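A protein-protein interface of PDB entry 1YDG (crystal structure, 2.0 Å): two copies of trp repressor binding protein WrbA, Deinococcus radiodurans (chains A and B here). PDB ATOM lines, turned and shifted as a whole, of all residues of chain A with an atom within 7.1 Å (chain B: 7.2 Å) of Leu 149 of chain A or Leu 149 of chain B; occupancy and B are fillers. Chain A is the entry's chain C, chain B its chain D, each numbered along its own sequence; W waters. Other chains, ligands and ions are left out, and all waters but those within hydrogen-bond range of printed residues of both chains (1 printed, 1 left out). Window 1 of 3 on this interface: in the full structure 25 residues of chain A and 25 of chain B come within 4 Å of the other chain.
Met 140 of chain A touches none of the printed residues of chain B. Of the printed residues of chain B, Leu 149 of chain A touches Val 148 and Leu 149. Of the printed residues of chain A, Met 143 of chain B touches Tyr 139 and Pro 151. Leu 149 of chain B touches just these residues of chain A: Ala 147, Val 148 and Leu 149. Of the printed residues of chain A, Pro 151 of chain B touches Met 143 and Ala 147. The nearest residue of chain A that does not touch Leu 149 of chain B is Met 143 of chain A (4.6 Å). The nearest printed residue of chain B that does not touch Val 148 of chain A is Leu 196 of chain B (4.03 Å).
N of Leu 149 of chain B lies within hydrogen-bond range of O of Leu 149 of chain A, 3.0 Å away. The guanidinium group (NH2) of Arg 192 of chain A sits at hydrogen-bond distance from the backbone carbonyl oxygen (O) of Gly 146 of chain B (2.7 Å). O of Gly 146 of chain A lies within hydrogen-bond range of NH2 of Arg 192 of chain B, at 2.7 Å.
Among the printed residues, pairs that only touch across the chains: Val 148 of chain A with Val 148 of chain B (3.3 Å), Leu 149 of chain A with Val 148 of chain B (3.4 Å), Val 148 of chain A with Leu 149 of chain B (3.6 Å), Tyr 139 of chain A with Met 143 of chain B (3.7 Å), Met 143 of chain A with Pro 151 of chain B (3.8 Å), Met 143 of chain A with Tyr 139 of chain B (3.8 Å), Pro 151 of chain A with Met 143 of chain B (3.9 Å), Ala 147 of chain A with Pro 151 of chain B (3.96 Å), Ala 147 of chain A with Leu 149 of chain B (3.98 Å) and Pro 151 of chain A with Ala 147 of chain B (3.99 Å).
Tyr 139 of chain A touches Met 143 of chain B, and with the chains exchanged Met 143 of chain A touches Tyr 139 of chain B. Met 143 of chain A touches Pro 151 of chain B, and with the chains exchanged Pro 151 of chain A touches Met 143 of chain B. Gly 146 of chain A touches Arg 192 of chain B, and with the chains exchanged Arg 192 of chain A touches Gly 146 of chain B. Val 148 of chain A touches Leu 149 of chain B, and with the chains exchanged Leu 149 of chain A touches Val 148 of chain B. 19 positions are printed for both chains. Of the 13 pairs that touch across the chains among the printed residues, 12 have their exchanged pair printed and touching as well.
Of the 19 printed residues of chain A, 8 touch a printed residue of chain B.
Water W1 lies within hydrogen-bond range of NH1 of Arg 192 of chain B (2.6 Å), O of Ala 147 of chain A (2.7 Å) and O of Pro 151 of chain B (2.9 Å).
The backbone NH (N) of Phe 118 of chain B sits at hydrogen-bond distance from the backbone carbonyl oxygen (O) of Val 148 of chain B, 3.0 Å away. O of Lys 116 of chain B is in hydrogen-bond range of N of Val 148 of chain B. The backbone carbonyl oxygen (O) of Lys 116 of chain A lies within hydrogen-bond range of the backbone NH (N) of Val 148 of chain A (2.8 Å). The backbone carbonyl oxygen (O) of Pro 151 of chain A lies within hydrogen-bond range of the guanidinium group (NH1) of Arg 192 of chain A, 2.6 Å away. O of Ala 142 of chain A lies within hydrogen-bond range of N of Ala 147 of chain A, at 3.2 Å. N of Ala 147 of chain B lies within hydrogen-bond range of O of Ala 142 of chain B (3.3 Å).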
ATOM      1  N   LYS A 116      13.963  12.947   1.535  1.00  0.00           N
ATOM      2  CA  LYS A 116      14.356  13.690   0.355  1.00  0.00           C
ATOM      3  C   LYS A 116      15.659  14.387   0.706  1.00  0.00           C
ATOM      4  O   LYS A 116      15.850  14.774   1.849  1.00  0.00           O
ATOM      5  CB  LYS A 116      13.264  14.689  -0.032  1.00  0.00           C
ATOM      6  CG  LYS A 116      11.965  13.999  -0.467  1.00  0.00           C
ATOM      7  CD  LYS A 116      10.825  14.966  -0.641  1.00  0.00           C
ATOM      8  CE  LYS A 116       9.507  14.238  -0.938  1.00  0.00           C
ATOM      9  NZ  LYS A 116       9.522  13.574  -2.250  1.00  0.00           N
ATOM     10  N   THR A 117      16.554  14.557  -0.263  1.00  0.00           N
ATOM     11  CA  THR A 117      17.775  15.330   0.003  1.00  0.00           C
ATOM     12  C   THR A 117      17.471  16.813  -0.038  1.00  0.00           C
ATOM     13  O   THR A 117      16.518  17.225  -0.684  1.00  0.00           O
ATOM     14  CB  THR A 117      18.941  14.985  -0.931  1.00  0.00           C
ATOM     15  OG1 THR A 117      18.602  15.264  -2.300  1.00  0.00           O
ATOM     16  CG2 THR A 117      19.340  13.511  -0.760  1.00  0.00           C
ATOM     17  N   PHE A 118      18.293  17.614   0.637  1.00  0.00           N
ATOM     18  CA  PHE A 118      18.048  19.048   0.746  1.00  0.00           C
ATOM     19  C   PHE A 118      19.330  19.821   0.915  1.00  0.00           C
ATOM     20  O   PHE A 118      20.174  19.507   1.767  1.00  0.00           O
ATOM     21  CB  PHE A 118      17.103  19.346   1.916  1.00  0.00           C
ATOM     22  CG  PHE A 118      16.762  20.817   2.092  1.00  0.00           C
ATOM     23  CD1 PHE A 118      15.622  21.354   1.533  1.00  0.00           C
ATOM     24  CD2 PHE A 118      17.585  21.655   2.842  1.00  0.00           C
ATOM     25  CE1 PHE A 118      15.301  22.703   1.721  1.00  0.00           C
ATOM     26  CE2 PHE A 118      17.277  23.002   3.029  1.00  0.00           C
ATOM     27  CZ  PHE A 118      16.139  23.527   2.459  1.00  0.00           C
ATOM     28  N   SER A 119      19.472  20.845   0.092  1.00  0.00           N
ATOM     29  CA  SER A 119      20.444  21.897   0.342  1.00  0.00           C
ATOM     30  C   SER A 119      19.809  23.246   0.028  1.00  0.00           C
ATOM     31  O   SER A 119      18.653  23.318  -0.410  1.00  0.00           O
ATOM     32  CB  SER A 119      21.705  21.681  -0.493  1.00  0.00           C
ATOM     33  OG  SER A 119      21.472  22.034  -1.838  1.00  0.00           O
ATOM     34  N   LEU A 138      16.922  27.777   6.837  1.00  0.00           N
ATOM     35  CA  LEU A 138      16.358  26.859   5.862  1.00  0.00           C
ATOM     36  C   LEU A 138      16.691  25.393   6.181  1.00  0.00           C
ATOM     37  O   LEU A 138      15.842  24.527   6.038  1.00  0.00           O
ATOM     38  CB  LEU A 138      16.810  27.231   4.456  1.00  0.00           C
ATOM     39  CG  LEU A 138      16.257  28.553   3.922  1.00  0.00           C
ATOM     40  CD1 LEU A 138      16.878  28.855   2.572  1.00  0.00           C
ATOM     41  CD2 LEU A 138      14.737  28.542   3.776  1.00  0.00           C
ATOM     42  N   TYR A 139      17.916  25.110   6.612  1.00  0.00           N
ATOM     43  CA  TYR A 139      18.244  23.747   7.035  1.00  0.00           C
ATOM     44  C   TYR A 139      17.419  23.284   8.254  1.00  0.00           C
ATOM     45  O   TYR A 139      16.925  22.152   8.287  1.00  0.00           O
ATOM     46  CB  TYR A 139      19.748  23.586   7.269  1.00  0.00           C
ATOM     47  CG  TYR A 139      20.559  23.554   5.983  1.00  0.00           C
ATOM     48  CD1 TYR A 139      20.491  22.477   5.126  1.00  0.00           C
ATOM     49  CD2 TYR A 139      21.389  24.622   5.627  1.00  0.00           C
ATOM     50  CE1 TYR A 139      21.241  22.427   3.950  1.00  0.00           C
ATOM     51  CE2 TYR A 139      22.134  24.602   4.450  1.00  0.00           C
ATOM     52  CZ  TYR A 139      22.058  23.491   3.609  1.00  0.00           C
ATOM     53  OH  TYR A 139      22.795  23.443   2.451  1.00  0.00           O
ATOM     54  N   MET A 140      17.242  24.156   9.241  1.00  0.00           N
ATOM     55  CA  MET A 140      16.457  23.784  10.420  1.00  0.00           C
ATOM     56  C   MET A 140      15.040  23.384  10.040  1.00  0.00           C
ATOM     57  O   MET A 140      14.510  22.420  10.586  1.00  0.00           O
ATOM     58  CB  MET A 140      16.440  24.895  11.478  1.00  0.00           C
ATOM     59  CG  MET A 140      17.825  25.271  12.049  1.00  0.00           C
ATOM     60  SD  MET A 140      19.036  23.929  12.222  1.00  0.00           S
ATOM     61  CE  MET A 140      18.685  23.312  13.887  1.00  0.00           C
ATOM     62  N   THR A 141      14.433  24.121   9.108  1.00  0.00           N
ATOM     63  CA  THR A 141      13.124  23.753   8.562  1.00  0.00           C
ATOM     64  C   THR A 141      13.116  22.368   7.909  1.00  0.00           C
ATOM     65  O   THR A 141      12.230  21.553   8.180  1.00  0.00           O
ATOM     66  CB  THR A 141      12.618  24.831   7.557  1.00  0.00           C
ATOM     67  OG1 THR A 141      12.221  25.991   8.288  1.00  0.00           O
ATOM     68  CG2 THR A 141      11.444  24.340   6.781  1.00  0.00           C
ATOM     69  N   ALA A 142      14.101  22.089   7.067  1.00  0.00           N
ATOM     70  CA  ALA A 142      14.198  20.775   6.426  1.00  0.00           C
ATOM     71  C   ALA A 142      14.363  19.596   7.414  1.00  0.00           C
ATOM     72  O   ALA A 142      13.931  18.466   7.135  1.00  0.00           O
ATOM     73  CB  ALA A 142      15.322  20.777   5.397  1.00  0.00           C
ATOM     74  N   MET A 143      14.969  19.857   8.564  1.00  0.00           N
ATOM     75  CA  MET A 143      15.076  18.840   9.636  1.00  0.00           C
ATOM     76  C   MET A 143      13.716  18.382  10.190  1.00  0.00           C
ATOM     77  O   MET A 143      13.562  17.219  10.551  1.00  0.00           O
ATOM     78  CB  MET A 143      15.910  19.372  10.803  1.00  0.00           C
ATOM     79  CG  MET A 143      17.346  19.679  10.433  1.00  0.00           C
ATOM     80  SD  MET A 143      18.378  19.759  11.878  1.00  0.00           S
ATOM     81  CE  MET A 143      19.872  20.432  11.163  1.00  0.00           C
ATOM     82  N   GLY A 146      12.440  15.572   8.211  1.00  0.00           N
ATOM     83  CA  GLY A 146      13.217  14.325   8.103  1.00  0.00           C
ATOM     84  C   GLY A 146      13.945  14.251   6.760  1.00  0.00           C
ATOM     85  O   GLY A 146      14.161  13.178   6.209  1.00  0.00           O
ATOM     86  N   ALA A 147      14.319  15.399   6.209  1.00  0.00           N
ATOM     87  CA  ALA A 147      15.093  15.414   4.977  1.00  0.00           C
ATOM     88  C   ALA A 147      16.526  15.003   5.284  1.00  0.00           C
ATOM     89  O   ALA A 147      16.947  15.017   6.436  1.00  0.00           O
ATOM     90  CB  ALA A 147      15.063  16.792   4.342  1.00  0.00           C
ATOM     91  N   VAL A 148      17.256  14.632   4.239  1.00  0.00           N
ATOM     92  CA  VAL A 148      18.649  14.231   4.320  1.00  0.00           C
ATOM     93  C   VAL A 148      19.415  15.427   3.790  1.00  0.00           C
ATOM     94  O   VAL A 148      19.349  15.741   2.600  1.00  0.00           O
ATOM     95  CB  VAL A 148      18.915  12.957   3.465  1.00  0.00           C
ATOM     96  CG1 VAL A 148      20.389  12.569   3.471  1.00  0.00           C
ATOM     97  CG2 VAL A 148      18.052  11.812   3.943  1.00  0.00           C
ATOM     98  N   LEU A 149      20.124  16.112   4.688  1.00  0.00           N
ATOM     99  CA  LEU A 149      20.771  17.392   4.344  1.00  0.00           C
ATOM    100  C   LEU A 149      22.146  17.143   3.737  1.00  0.00           C
ATOM    101  O   LEU A 149      22.985  16.445   4.325  1.00  0.00           O
ATOM    102  CB  LEU A 149      20.868  18.323   5.568  1.00  0.00           C
ATOM    103  CG  LEU A 149      19.640  18.419   6.483  1.00  0.00           C
ATOM    104  CD1 LEU A 149      19.799  19.514   7.563  1.00  0.00           C
ATOM    105  CD2 LEU A 149      18.366  18.640   5.683  1.00  0.00           C
ATOM    106  N   THR A 150      22.358  17.731   2.557  1.00  0.00           N
ATOM    107  CA  THR A 150      23.568  17.561   1.776  1.00  0.00           C
ATOM    108  C   THR A 150      24.221  18.911   1.453  1.00  0.00           C
ATOM    109  O   THR A 150      24.362  19.282   0.289  1.00  0.00           O
ATOM    110  CB  THR A 150      23.274  16.799   0.463  1.00  0.00           C
ATOM    111  OG1 THR A 150      22.435  17.569  -0.415  1.00  0.00           O
ATOM    112  CG2 THR A 150      22.587  15.489   0.758  1.00  0.00           C
ATOM    113  N   PRO A 151      24.671  19.632   2.487  1.00  0.00           N
ATOM    114  CA  PRO A 151      25.400  20.853   2.241  1.00  0.00           C
ATOM    115  C   PRO A 151      26.746  20.570   1.561  1.00  0.00           C
ATOM    116  O   PRO A 151      27.270  19.455   1.666  1.00  0.00           O
ATOM    117  CB  PRO A 151      25.628  21.409   3.658  1.00  0.00           C
ATOM    118  CG  PRO A 151      25.641  20.187   4.510  1.00  0.00           C
ATOM    119  CD  PRO A 151      24.571  19.347   3.929  1.00  0.00           C
ATOM    120  N   ARG A 192      27.029  17.429  -6.508  1.00  0.00           N
ATOM    121  CA  ARG A 192      27.227  16.598  -5.321  1.00  0.00           C
ATOM    122  C   ARG A 192      25.915  16.014  -4.805  1.00  0.00           C
ATOM    123  O   ARG A 192      25.820  14.820  -4.541  1.00  0.00           O
ATOM    124  CB  ARG A 192      27.894  17.434  -4.221  1.00  0.00           C
ATOM    125  CG  ARG A 192      27.989  16.736  -2.866  1.00  0.00           C
ATOM    126  CD  ARG A 192      29.155  17.272  -2.044  1.00  0.00           C
ATOM    127  NE  ARG A 192      29.452  16.399  -0.896  1.00  0.00           N
ATOM    128  CZ  ARG A 192      28.753  16.440   0.221  1.00  0.00           C
ATOM    129  NH1 ARG A 192      27.738  17.279   0.307  1.00  0.00           N
ATOM    130  NH2 ARG A 192      29.028  15.636   1.232  1.00  0.00           N
ATOM    131  N   GLN A 193      24.906  16.870  -4.654  1.00  0.00           N
ATOM    132  CA  GLN A 193      23.611  16.444  -4.128  1.00  0.00           C
ATOM    133  C   GLN A 193      22.914  15.458  -5.051  1.00  0.00           C
ATOM    134  O   GLN A 193      22.331  14.479  -4.577  1.00  0.00           O
ATOM    135  CB  GLN A 193      22.711  17.650  -3.807  1.00  0.00           C
ATOM    136  CG  GLN A 193      21.276  17.273  -3.417  1.00  0.00           C
ATOM    137  CD  GLN A 193      20.444  18.452  -2.953  1.00  0.00           C
ATOM    138  OE1 GLN A 193      19.291  18.285  -2.542  1.00  0.00           O
ATOM    139  NE2 GLN A 193      21.003  19.638  -3.029  1.00  0.00           N
ATOM    140  N   LEU A 196      24.745  12.071  -4.459  1.00  0.00           N
ATOM    141  CA  LEU A 196      24.325  11.452  -3.188  1.00  0.00           C
ATOM    142  C   LEU A 196      22.882  10.899  -3.273  1.00  0.00           C
ATOM    143  O   LEU A 196      22.594   9.769  -2.842  1.00  0.00           O
ATOM    144  CB  LEU A 196      24.468  12.432  -2.010  1.00  0.00           C
ATOM    145  CG  LEU A 196      25.885  12.913  -1.663  1.00  0.00           C
ATOM    146  CD1 LEU A 196      25.847  14.149  -0.812  1.00  0.00           C
ATOM    147  CD2 LEU A 196      26.683  11.820  -0.965  1.00  0.00           C
ATOM    148  N   LYS B 116      30.224  10.980   5.507  1.00  0.00           N
ATOM    149  CA  LYS B 116      29.730  10.201   6.622  1.00  0.00           C
ATOM    150  C   LYS B 116      28.393  10.797   7.038  1.00  0.00           C
ATOM    151  O   LYS B 116      28.196  12.016   6.936  1.00  0.00           O
ATOM    152  CB  LYS B 116      30.717  10.242   7.795  1.00  0.00           C
ATOM    153  CG  LYS B 116      32.064   9.603   7.465  1.00  0.00           C
ATOM    154  CD  LYS B 116      33.075   9.825   8.556  1.00  0.00           C
ATOM    155  CE  LYS B 116      34.501   9.685   8.042  1.00  0.00           C
ATOM    156  NZ  LYS B 116      34.849   8.287   7.712  1.00  0.00           N
ATOM    157  N   THR B 117      27.474   9.947   7.488  1.00  0.00           N
ATOM    158  CA  THR B 117      26.217  10.440   8.049  1.00  0.00           C
ATOM    159  C   THR B 117      26.419  10.983   9.476  1.00  0.00           C
ATOM    160  O   THR B 117      27.253  10.509  10.223  1.00  0.00           O
ATOM    161  CB  THR B 117      25.094   9.375   8.036  1.00  0.00           C
ATOM    162  OG1 THR B 117      25.488   8.243   8.815  1.00  0.00           O
ATOM    163  CG2 THR B 117      24.796   8.928   6.604  1.00  0.00           C
ATOM    164  N   PHE B 118      25.640  11.990   9.836  1.00  0.00           N
ATOM    165  CA  PHE B 118      25.742  12.581  11.154  1.00  0.00           C
ATOM    166  C   PHE B 118      24.375  12.885  11.745  1.00  0.00           C
ATOM    167  O   PHE B 118      23.509  13.447  11.063  1.00  0.00           O
ATOM    168  CB  PHE B 118      26.554  13.877  11.043  1.00  0.00           C
ATOM    169  CG  PHE B 118      26.796  14.561  12.359  1.00  0.00           C
ATOM    170  CD1 PHE B 118      27.901  14.233  13.130  1.00  0.00           C
ATOM    171  CD2 PHE B 118      25.932  15.534  12.815  1.00  0.00           C
ATOM    172  CE1 PHE B 118      28.127  14.858  14.327  1.00  0.00           C
ATOM    173  CE2 PHE B 118      26.148  16.165  14.026  1.00  0.00           C
ATOM    174  CZ  PHE B 118      27.244  15.822  14.788  1.00  0.00           C
ATOM    175  N   SER B 119      24.223  12.567  13.023  1.00  0.00           N
ATOM    176  CA  SER B 119      23.137  13.096  13.845  1.00  0.00           C
ATOM    177  C   SER B 119      23.644  13.358  15.237  1.00  0.00           C
ATOM    178  O   SER B 119      24.773  13.015  15.562  1.00  0.00           O
ATOM    179  CB  SER B 119      21.926  12.145  13.875  1.00  0.00           C
ATOM    180  OG  SER B 119      22.170  10.974  14.636  1.00  0.00           O
ATOM    181  N   LEU B 138      26.052  21.446  16.862  1.00  0.00           N
ATOM    182  CA  LEU B 138      26.739  20.226  16.462  1.00  0.00           C
ATOM    183  C   LEU B 138      26.509  19.915  14.978  1.00  0.00           C
ATOM    184  O   LEU B 138      27.431  19.543  14.277  1.00  0.00           O
ATOM    185  CB  LEU B 138      26.317  19.059  17.351  1.00  0.00           C
ATOM    186  CG  LEU B 138      26.730  19.142  18.828  1.00  0.00           C
ATOM    187  CD1 LEU B 138      25.986  18.073  19.668  1.00  0.00           C
ATOM    188  CD2 LEU B 138      28.250  19.023  18.984  1.00  0.00           C
ATOM    189  N   TYR B 139      25.281  20.088  14.510  1.00  0.00           N
ATOM    190  CA  TYR B 139      24.970  19.966  13.095  1.00  0.00           C
ATOM    191  C   TYR B 139      25.721  20.993  12.246  1.00  0.00           C
ATOM    192  O   TYR B 139      26.258  20.653  11.197  1.00  0.00           O
ATOM    193  CB  TYR B 139      23.465  20.088  12.846  1.00  0.00           C
ATOM    194  CG  TYR B 139      22.686  18.864  13.235  1.00  0.00           C
ATOM    195  CD1 TYR B 139      22.824  17.676  12.529  1.00  0.00           C
ATOM    196  CD2 TYR B 139      21.823  18.880  14.317  1.00  0.00           C
ATOM    197  CE1 TYR B 139      22.128  16.564  12.884  1.00  0.00           C
ATOM    198  CE2 TYR B 139      21.110  17.756  14.678  1.00  0.00           C
ATOM    199  CZ  TYR B 139      21.264  16.604  13.951  1.00  0.00           C
ATOM    200  OH  TYR B 139      20.570  15.468  14.308  1.00  0.00           O
ATOM    201  N   MET B 140      25.781  22.243  12.701  1.00  0.00           N
ATOM    202  CA  MET B 140      26.498  23.265  11.932  1.00  0.00           C
ATOM    203  C   MET B 140      27.956  22.872  11.738  1.00  0.00           C
ATOM    204  O   MET B 140      28.485  22.998  10.646  1.00  0.00           O
ATOM    205  CB  MET B 140      26.348  24.660  12.560  1.00  0.00           C
ATOM    206  CG  MET B 140      24.918  25.238  12.481  1.00  0.00           C
ATOM    207  SD  MET B 140      23.961  24.983  10.961  1.00  0.00           S
ATOM    208  CE  MET B 140      24.516  26.337   9.904  1.00  0.00           C
ATOM    209  N   THR B 141      28.584  22.359  12.787  1.00  0.00           N
ATOM    210  CA  THR B 141      29.945  21.810  12.716  1.00  0.00           C
ATOM    211  C   THR B 141      30.088  20.700  11.676  1.00  0.00           C
ATOM    212  O   THR B 141      31.003  20.727  10.868  1.00  0.00           O
ATOM    213  CB  THR B 141      30.392  21.313  14.117  1.00  0.00           C
ATOM    214  OG1 THR B 141      30.619  22.450  14.940  1.00  0.00           O
ATOM    215  CG2 THR B 141      31.648  20.456  14.070  1.00  0.00           C
ATOM    216  N   ALA B 142      29.171  19.736  11.695  1.00  0.00           N
ATOM    217  CA  ALA B 142      29.195  18.641  10.741  1.00  0.00           C
ATOM    218  C   ALA B 142      29.124  19.108   9.291  1.00  0.00           C
ATOM    219  O   ALA B 142      29.674  18.460   8.396  1.00  0.00           O
ATOM    220  CB  ALA B 142      28.052  17.669  11.026  1.00  0.00           C
ATOM    221  N   MET B 143      28.423  20.209   9.050  1.00  0.00           N
ATOM    222  CA  MET B 143      28.346  20.766   7.702  1.00  0.00           C
ATOM    223  C   MET B 143      29.714  21.212   7.159  1.00  0.00           C
ATOM    224  O   MET B 143      29.962  21.109   5.950  1.00  0.00           O
ATOM    225  CB  MET B 143      27.392  21.944   7.671  1.00  0.00           C
ATOM    226  CG  MET B 143      25.938  21.650   8.105  1.00  0.00           C
ATOM    227  SD  MET B 143      24.815  22.935   7.451  1.00  0.00           S
ATOM    228  CE  MET B 143      23.293  22.602   8.310  1.00  0.00           C
ATOM    229  N   GLY B 146      31.353  18.334   5.370  1.00  0.00           N
ATOM    230  CA  GLY B 146      30.695  17.720   4.231  1.00  0.00           C
ATOM    231  C   GLY B 146      29.958  16.439   4.617  1.00  0.00           C
ATOM    232  O   GLY B 146      29.868  15.487   3.836  1.00  0.00           O
ATOM    233  N   ALA B 147      29.454  16.400   5.848  1.00  0.00           N
ATOM    234  CA  ALA B 147      28.710  15.247   6.326  1.00  0.00           C
ATOM    235  C   ALA B 147      27.319  15.326   5.750  1.00  0.00           C
ATOM    236  O   ALA B 147      26.865  16.401   5.347  1.00  0.00           O
ATOM    237  CB  ALA B 147      28.664  15.232   7.856  1.00  0.00           C
ATOM    238  N   VAL B 148      26.657  14.178   5.695  1.00  0.00           N
ATOM    239  CA  VAL B 148      25.272  14.060   5.263  1.00  0.00           C
ATOM    240  C   VAL B 148      24.464  13.961   6.542  1.00  0.00           C
ATOM    241  O   VAL B 148      24.576  12.962   7.247  1.00  0.00           O
ATOM    242  CB  VAL B 148      25.070  12.782   4.420  1.00  0.00           C
ATOM    243  CG1 VAL B 148      23.596  12.574   4.061  1.00  0.00           C
ATOM    244  CG2 VAL B 148      25.929  12.817   3.191  1.00  0.00           C
ATOM    245  N   LEU B 149      23.643  14.976   6.843  1.00  0.00           N
ATOM    246  CA  LEU B 149      22.970  15.047   8.140  1.00  0.00           C
ATOM    247  C   LEU B 149      21.647  14.300   8.115  1.00  0.00           C
ATOM    248  O   LEU B 149      20.815  14.555   7.239  1.00  0.00           O
ATOM    249  CB  LEU B 149      22.723  16.490   8.548  1.00  0.00           C
ATOM    250  CG  LEU B 149      23.886  17.473   8.349  1.00  0.00           C
ATOM    251  CD1 LEU B 149      23.520  18.803   8.955  1.00  0.00           C
ATOM    252  CD2 LEU B 149      25.202  16.947   8.915  1.00  0.00           C
ATOM    253  N   THR B 150      21.455  13.406   9.092  1.00  0.00           N
ATOM    254  CA  THR B 150      20.279  12.528   9.159  1.00  0.00           C
ATOM    255  C   THR B 150      19.510  12.733  10.494  1.00  0.00           C
ATOM    256  O   THR B 150      19.379  11.806  11.279  1.00  0.00           O
ATOM    257  CB  THR B 150      20.673  11.037   9.014  1.00  0.00           C
ATOM    258  OG1 THR B 150      21.540  10.653  10.090  1.00  0.00           O
ATOM    259  CG2 THR B 150      21.386  10.764   7.673  1.00  0.00           C
ATOM    260  N   PRO B 151      18.967  13.942  10.724  1.00  0.00           N
ATOM    261  CA  PRO B 151      18.205  14.197  11.924  1.00  0.00           C
ATOM    262  C   PRO B 151      16.939  13.338  11.893  1.00  0.00           C
ATOM    263  O   PRO B 151      16.520  12.906  10.816  1.00  0.00           O
ATOM    264  CB  PRO B 151      17.878  15.685  11.812  1.00  0.00           C
ATOM    265  CG  PRO B 151      17.815  15.913  10.339  1.00  0.00           C
ATOM    266  CD  PRO B 151      18.969  15.114   9.839  1.00  0.00           C
ATOM    267  N   ARG B 192      17.089   4.622  12.036  1.00  0.00           N
ATOM    268  CA  ARG B 192      16.925   5.373  10.814  1.00  0.00           C
ATOM    269  C   ARG B 192      18.266   5.783  10.193  1.00  0.00           C
ATOM    270  O   ARG B 192      18.479   5.598   9.002  1.00  0.00           O
ATOM    271  CB  ARG B 192      16.065   6.588  11.106  1.00  0.00           C
ATOM    272  CG  ARG B 192      15.932   7.534   9.965  1.00  0.00           C
ATOM    273  CD  ARG B 192      14.800   8.512  10.223  1.00  0.00           C
ATOM    274  NE  ARG B 192      14.518   9.242   8.996  1.00  0.00           N
ATOM    275  CZ  ARG B 192      15.255  10.246   8.563  1.00  0.00           C
ATOM    276  NH1 ARG B 192      16.308  10.642   9.264  1.00  0.00           N
ATOM    277  NH2 ARG B 192      14.956  10.846   7.429  1.00  0.00           N
ATOM    278  N   GLN B 193      19.178   6.321  10.998  1.00  0.00           N
ATOM    279  CA  GLN B 193      20.497   6.710  10.479  1.00  0.00           C
ATOM    280  C   GLN B 193      21.257   5.508   9.908  1.00  0.00           C
ATOM    281  O   GLN B 193      21.840   5.595   8.843  1.00  0.00           O
ATOM    282  CB  GLN B 193      21.347   7.394  11.552  1.00  0.00           C
ATOM    283  CG  GLN B 193      22.720   7.790  11.048  1.00  0.00           C
ATOM    284  CD  GLN B 193      23.467   8.733  11.957  1.00  0.00           C
ATOM    285  OE1 GLN B 193      24.604   9.090  11.655  1.00  0.00           O
ATOM    286  NE2 GLN B 193      22.860   9.126  13.080  1.00  0.00           N
ATOM    287  N   LEU B 196      19.658   4.591   6.488  1.00  0.00           N
ATOM    288  CA  LEU B 196      20.064   5.544   5.454  1.00  0.00           C
ATOM    289  C   LEU B 196      21.514   5.352   5.036  1.00  0.00           C
ATOM    290  O   LEU B 196      21.826   5.409   3.844  1.00  0.00           O
ATOM    291  CB  LEU B 196      19.862   6.988   5.923  1.00  0.00           C
ATOM    292  CG  LEU B 196      18.425   7.530   5.943  1.00  0.00           C
ATOM    293  CD1 LEU B 196      18.342   8.759   6.824  1.00  0.00           C
ATOM    294  CD2 LEU B 196      17.894   7.832   4.551  1.00  0.00           C
HETATM  295  O   HOH W   1      17.133  12.786   8.030  1.00  0.00           O
